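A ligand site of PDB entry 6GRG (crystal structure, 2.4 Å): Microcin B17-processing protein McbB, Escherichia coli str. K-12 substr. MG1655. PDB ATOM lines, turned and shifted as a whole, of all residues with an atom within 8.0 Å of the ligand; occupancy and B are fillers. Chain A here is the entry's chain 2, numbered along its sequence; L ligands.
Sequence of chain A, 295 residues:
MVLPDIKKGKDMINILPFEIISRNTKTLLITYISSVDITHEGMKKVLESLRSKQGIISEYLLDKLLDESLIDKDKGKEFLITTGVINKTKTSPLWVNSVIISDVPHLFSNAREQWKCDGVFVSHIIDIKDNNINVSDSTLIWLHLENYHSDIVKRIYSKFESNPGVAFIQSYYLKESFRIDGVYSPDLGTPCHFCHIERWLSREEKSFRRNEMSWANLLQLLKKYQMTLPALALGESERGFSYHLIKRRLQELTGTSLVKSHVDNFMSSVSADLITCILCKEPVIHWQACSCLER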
ATOM      1  N   ILE A  13     -24.034  20.748 -26.548  1.00  0.00           N
ATOM      2  CA  ILE A  13     -23.630  19.439 -25.917  1.00  0.00           C
ATOM      3  C   ILE A  13     -22.257  19.016 -26.465  1.00  0.00           C
ATOM      4  O   ILE A  13     -22.115  18.830 -27.646  1.00  0.00           O
ATOM      5  CB  ILE A  13     -24.665  18.324 -26.181  1.00  0.00           C
ATOM      6  CG1 ILE A  13     -26.111  18.770 -25.924  1.00  0.00           C
ATOM      7  CG2 ILE A  13     -24.312  17.067 -25.372  1.00  0.00           C
ATOM      8  CD1 ILE A  13     -26.422  19.138 -24.479  1.00  0.00           C
ATOM      9  N   ILE A  56     -18.924  17.038 -29.929  1.00  0.00           N
ATOM     10  CA  ILE A  56     -20.116  17.944 -30.092  1.00  0.00           C
ATOM     11  C   ILE A  56     -21.292  17.250 -30.847  1.00  0.00           C
ATOM     12  O   ILE A  56     -21.132  16.740 -31.941  1.00  0.00           O
ATOM     13  CB  ILE A  56     -19.685  19.275 -30.769  1.00  0.00           C
ATOM     14  CG1 ILE A  56     -18.761  20.132 -29.886  1.00  0.00           C
ATOM     15  CG2 ILE A  56     -20.881  20.076 -31.256  1.00  0.00           C
ATOM     16  CD1 ILE A  56     -19.467  20.965 -28.833  1.00  0.00           C
ATOM     17  N   ILE A  57     -22.470  17.273 -30.215  1.00  0.00           N
ATOM     18  CA  ILE A  57     -23.784  16.803 -30.707  1.00  0.00           C
ATOM     19  C   ILE A  57     -24.810  17.907 -30.404  1.00  0.00           C
ATOM     20  O   ILE A  57     -24.534  18.830 -29.612  1.00  0.00           O
ATOM     21  CB  ILE A  57     -24.175  15.466 -30.042  1.00  0.00           C
ATOM     22  CG1 ILE A  57     -25.314  14.746 -30.764  1.00  0.00           C
ATOM     23  CG2 ILE A  57     -24.517  15.660 -28.567  1.00  0.00           C
ATOM     24  CD1 ILE A  57     -25.903  13.573 -29.993  1.00  0.00           C
ATOM     25  N   SER A  58     -25.997  17.824 -31.022  1.00  0.00           N
ATOM     26  CA  SER A  58     -27.135  18.712 -30.728  1.00  0.00           C
ATOM     27  C   SER A  58     -28.071  18.099 -29.669  1.00  0.00           C
ATOM     28  O   SER A  58     -28.393  16.903 -29.713  1.00  0.00           O
ATOM     29  CB  SER A  58     -27.905  19.025 -31.981  1.00  0.00           C
ATOM     30  OG  SER A  58     -28.777  17.948 -32.312  1.00  0.00           O
ATOM     31  N   GLU A  59     -28.543  18.976 -28.766  1.00  0.00           N
ATOM     32  CA  GLU A  59     -29.660  18.730 -27.830  1.00  0.00           C
ATOM     33  C   GLU A  59     -30.792  17.966 -28.521  1.00  0.00           C
ATOM     34  O   GLU A  59     -31.351  17.076 -27.909  1.00  0.00           O
ATOM     35  CB  GLU A  59     -30.197  20.044 -27.253  1.00  0.00           C
ATOM     36  CG  GLU A  59     -29.594  20.429 -25.909  1.00  0.00           C
ATOM     37  CD  GLU A  59     -30.303  19.829 -24.698  1.00  0.00           C
ATOM     38  OE1 GLU A  59     -30.785  18.689 -24.797  1.00  0.00           O
ATOM     39  OE2 GLU A  59     -30.397  20.525 -23.663  1.00  0.00           O
ATOM     40  N   TYR A  60     -31.120  18.299 -29.770  1.00  0.00           N
ATOM     41  CA  TYR A  60     -32.215  17.623 -30.482  1.00  0.00           C
ATOM     42  C   TYR A  60     -31.850  16.146 -30.724  1.00  0.00           C
ATOM     43  O   TYR A  60     -32.693  15.257 -30.496  1.00  0.00           O
ATOM     44  CB  TYR A  60     -32.592  18.363 -31.766  1.00  0.00           C
ATOM     45  CG  TYR A  60     -33.479  17.585 -32.723  1.00  0.00           C
ATOM     46  CD1 TYR A  60     -32.918  16.816 -33.746  1.00  0.00           C
ATOM     47  CD2 TYR A  60     -34.855  17.598 -32.614  1.00  0.00           C
ATOM     48  CE1 TYR A  60     -33.715  16.087 -34.613  1.00  0.00           C
ATOM     49  CE2 TYR A  60     -35.670  16.879 -33.487  1.00  0.00           C
ATOM     50  CZ  TYR A  60     -35.091  16.119 -34.488  1.00  0.00           C
ATOM     51  OH  TYR A  60     -35.857  15.410 -35.360  1.00  0.00           O
ATOM     52  N   LEU A  61     -30.622  15.865 -31.183  1.00  0.00           N
ATOM     53  CA  LEU A  61     -30.288  14.468 -31.508  1.00  0.00           C
ATOM     54  C   LEU A  61     -30.212  13.624 -30.222  1.00  0.00           C
ATOM     55  O   LEU A  61     -30.746  12.510 -30.220  1.00  0.00           O
ATOM     56  CB  LEU A  61     -29.004  14.345 -32.332  1.00  0.00           C
ATOM     57  CG  LEU A  61     -28.955  13.057 -33.169  1.00  0.00           C
ATOM     58  CD1 LEU A  61     -29.684  13.243 -34.505  1.00  0.00           C
ATOM     59  CD2 LEU A  61     -27.526  12.565 -33.385  1.00  0.00           C
ATOM     60  N   LEU A  62     -29.609  14.165 -29.160  1.00  0.00           N
ATOM     61  CA  LEU A  62     -29.567  13.497 -27.820  1.00  0.00           C
ATOM     62  C   LEU A  62     -30.977  13.114 -27.352  1.00  0.00           C
ATOM     63  O   LEU A  62     -31.215  11.979 -26.900  1.00  0.00           O
ATOM     64  CB  LEU A  62     -28.889  14.433 -26.808  1.00  0.00           C
ATOM     65  CG  LEU A  62     -28.831  13.936 -25.355  1.00  0.00           C
ATOM     66  CD1 LEU A  62     -28.340  12.491 -25.264  1.00  0.00           C
ATOM     67  CD2 LEU A  62     -27.936  14.838 -24.512  1.00  0.00           C
ATOM     68  N   ASP A  63     -31.913  14.073 -27.447  1.00  0.00           N
ATOM     69  CA  ASP A  63     -33.301  13.873 -27.028  1.00  0.00           C
ATOM     70  C   ASP A  63     -33.928  12.785 -27.882  1.00  0.00           C
ATOM     71  O   ASP A  63     -34.691  11.981 -27.357  1.00  0.00           O
ATOM     72  CB  ASP A  63     -34.097  15.175 -27.085  1.00  0.00           C
ATOM     73  CG  ASP A  63     -33.822  16.128 -25.925  1.00  0.00           C
ATOM     74  OD1 ASP A  63     -32.828  15.909 -25.211  1.00  0.00           O
ATOM     75  OD2 ASP A  63     -34.605  17.070 -25.730  1.00  0.00           O
ATOM     76  N   LYS A  88     -22.793  20.695 -21.077  1.00  0.00           N
ATOM     77  CA  LYS A  88     -23.792  21.518 -21.738  1.00  0.00           C
ATOM     78  C   LYS A  88     -23.153  22.882 -22.062  1.00  0.00           C
ATOM     79  O   LYS A  88     -23.408  23.860 -21.367  1.00  0.00           O
ATOM     80  CB  LYS A  88     -24.992  21.614 -20.779  1.00  0.00           C
ATOM     81  CG  LYS A  88     -26.369  21.816 -21.395  1.00  0.00           C
ATOM     82  CD  LYS A  88     -27.461  21.207 -20.517  1.00  0.00           C
ATOM     83  CE  LYS A  88     -28.685  22.067 -20.360  1.00  0.00           C
ATOM     84  NZ  LYS A  88     -29.200  22.520 -21.679  1.00  0.00           N
ATOM     85  N   THR A  89     -22.334  22.930 -23.131  1.00  0.00           N
ATOM     86  CA  THR A  89     -21.372  24.041 -23.392  1.00  0.00           C
ATOM     87  C   THR A  89     -21.934  25.087 -24.370  1.00  0.00           C
ATOM     88  O   THR A  89     -22.820  24.797 -25.179  1.00  0.00           O
ATOM     89  CB  THR A  89     -20.041  23.500 -23.926  1.00  0.00           C
ATOM     90  OG1 THR A  89     -19.097  24.565 -23.847  1.00  0.00           O
ATOM     91  CG2 THR A  89     -20.133  22.970 -25.338  1.00  0.00           C
ATOM     92  N   LYS A  90     -21.387  26.305 -24.306  1.00  0.00           N
ATOM     93  CA  LYS A  90     -21.881  27.484 -25.069  1.00  0.00           C
ATOM     94  C   LYS A  90     -21.243  27.549 -26.469  1.00  0.00           C
ATOM     95  O   LYS A  90     -20.022  27.428 -26.621  1.00  0.00           O
ATOM     96  CB  LYS A  90     -21.569  28.786 -24.320  1.00  0.00           C
ATOM     97  CG  LYS A  90     -22.769  29.421 -23.632  1.00  0.00           C
ATOM     98  CD  LYS A  90     -22.460  30.742 -22.961  1.00  0.00           C
ATOM     99  CE  LYS A  90     -23.727  31.408 -22.460  1.00  0.00           C
ATOM    100  NZ  LYS A  90     -23.424  32.745 -21.897  1.00  0.00           N
ATOM    101  N   THR A  91     -22.097  27.803 -27.487  1.00  0.00           N
ATOM    102  CA  THR A  91     -21.665  28.090 -28.869  1.00  0.00           C
ATOM    103  C   THR A  91     -21.137  29.540 -28.985  1.00  0.00           C
ATOM    104  O   THR A  91     -20.366  29.850 -29.907  1.00  0.00           O
ATOM    105  CB  THR A  91     -22.783  27.765 -29.876  1.00  0.00           C
ATOM    106  OG1 THR A  91     -23.992  28.476 -29.592  1.00  0.00           O
ATOM    107  CG2 THR A  91     -23.090  26.288 -29.917  1.00  0.00           C
ATOM    108  N   SER A  92     -21.537  30.418 -28.043  1.00  0.00           N
ATOM    109  CA  SER A  92     -21.011  31.799 -27.949  1.00  0.00           C
ATOM    110  C   SER A  92     -19.838  31.820 -26.975  1.00  0.00           C
ATOM    111  O   SER A  92     -19.592  30.827 -26.295  1.00  0.00           O
ATOM    112  CB  SER A  92     -22.103  32.752 -27.537  1.00  0.00           C
ATOM    113  OG  SER A  92     -22.202  32.820 -26.129  1.00  0.00           O
ATOM    114  N   VAL A 259     -17.129  25.627 -29.917  1.00  0.00           N
ATOM    115  CA  VAL A 259     -17.417  25.604 -31.387  1.00  0.00           C
ATOM    116  C   VAL A 259     -16.313  26.374 -32.145  1.00  0.00           C
ATOM    117  O   VAL A 259     -15.793  25.868 -33.134  1.00  0.00           O
ATOM    118  CB  VAL A 259     -18.836  26.086 -31.791  1.00  0.00           C
ATOM    119  CG1 VAL A 259     -19.911  25.067 -31.444  1.00  0.00           C
ATOM    120  CG2 VAL A 259     -19.192  27.466 -31.243  1.00  0.00           C
HETATM  121  P1  LIG L   1     -27.328  26.456 -28.627  1.00  0.00           P
HETATM  122  O1  LIG L   1     -27.864  26.024 -27.277  1.00  0.00           O
HETATM  123  O2  LIG L   1     -25.851  26.785 -28.657  1.00  0.00           O
HETATM  124  O3  LIG L   1     -28.157  27.577 -29.211  1.00  0.00           O
HETATM  125  P2  LIG L   1     -28.234  23.774 -29.571  1.00  0.00           P
HETATM  126  O4  LIG L   1     -27.717  22.893 -30.702  1.00  0.00           O
HETATM  127  O5  LIG L   1     -28.110  23.285 -28.149  1.00  0.00           O
HETATM  128  O6  LIG L   1     -27.510  25.249 -29.717  1.00  0.00           O
HETATM  129  P3  LIG L   1     -30.759  22.766 -30.389  1.00  0.00           P
HETATM  130  O7  LIG L   1     -30.071  21.439 -30.140  1.00  0.00           O
HETATM  131  O8  LIG L   1     -32.150  23.008 -29.853  1.00  0.00           O
HETATM  132  O9  LIG L   1     -29.810  23.979 -29.873  1.00  0.00           O
HETATM  133  O10 LIG L   1     -30.804  22.972 -31.984  1.00  0.00           O
HETATM  134  C1  LIG L   1     -30.313  22.004 -32.930  1.00  0.00           C
HETATM  135  C2  LIG L   1     -31.130  21.962 -34.226  1.00  0.00           C
HETATM  136  O11 LIG L   1     -32.106  20.902 -34.159  1.00  0.00           O
HETATM  137  C3  LIG L   1     -31.908  23.241 -34.567  1.00  0.00           C
HETATM  138  O12 LIG L   1     -31.121  24.152 -35.365  1.00  0.00           O
HETATM  139  C4  LIG L   1     -33.172  22.725 -35.267  1.00  0.00           C
HETATM  140  O13 LIG L   1     -33.049  22.763 -36.691  1.00  0.00           O
HETATM  141  C5  LIG L   1     -33.331  21.277 -34.810  1.00  0.00           C
HETATM  142  N1  LIG L   1     -34.491  21.130 -33.870  1.00  0.00           N
HETATM  143  C6  LIG L   1     -34.512  21.440 -32.549  1.00  0.00           C
HETATM  144  N2  LIG L   1     -35.730  21.164 -32.009  1.00  0.00           N
HETATM  145  C7  LIG L   1     -36.512  20.670 -32.993  1.00  0.00           C
HETATM  146  C8  LIG L   1     -37.917  20.182 -33.117  1.00  0.00           C
HETATM  147  N3  LIG L   1     -38.737  20.178 -32.038  1.00  0.00           N
HETATM  148  N4  LIG L   1     -38.338  19.746 -34.333  1.00  0.00           N
HETATM  149  C9  LIG L   1     -37.532  19.748 -35.423  1.00  0.00           C
HETATM  150  N5  LIG L   1     -36.261  20.182 -35.371  1.00  0.00           N
HETATM  151  C10 LIG L   1     -35.695  20.642 -34.225  1.00  0.00           C
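Ser 58 touches the ligand (CB to O7, 3.7 Å).
Four residues have an atom within 4 Å of the ligand: Ser 58, Glu 59, Tyr 60 and Thr 91.
OG1 of Thr 91 is in hydrogen-bond range of O2 of the ligand.
An oxygen (O7) of the ligand sits at hydrogen-bond distance from the backbone NH (N) of Glu 59 (3.2 Å).
The backbone NH (N) of Tyr 60 is in hydrogen-bond range of an oxygen (O7) of the ligand (3.3 Å).
NZ of Lys 88 lies within salt-bridge range of OE2 of Glu 59, 3.1 Å away.
N of Leu 61 is in hydrogen-bond range of OG of Ser 58, 3.0 Å away.
The backbone NH (N) of Tyr 60 sits close to the side-chain hydroxyl (OG) of Ser 58 (3.5 Å).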
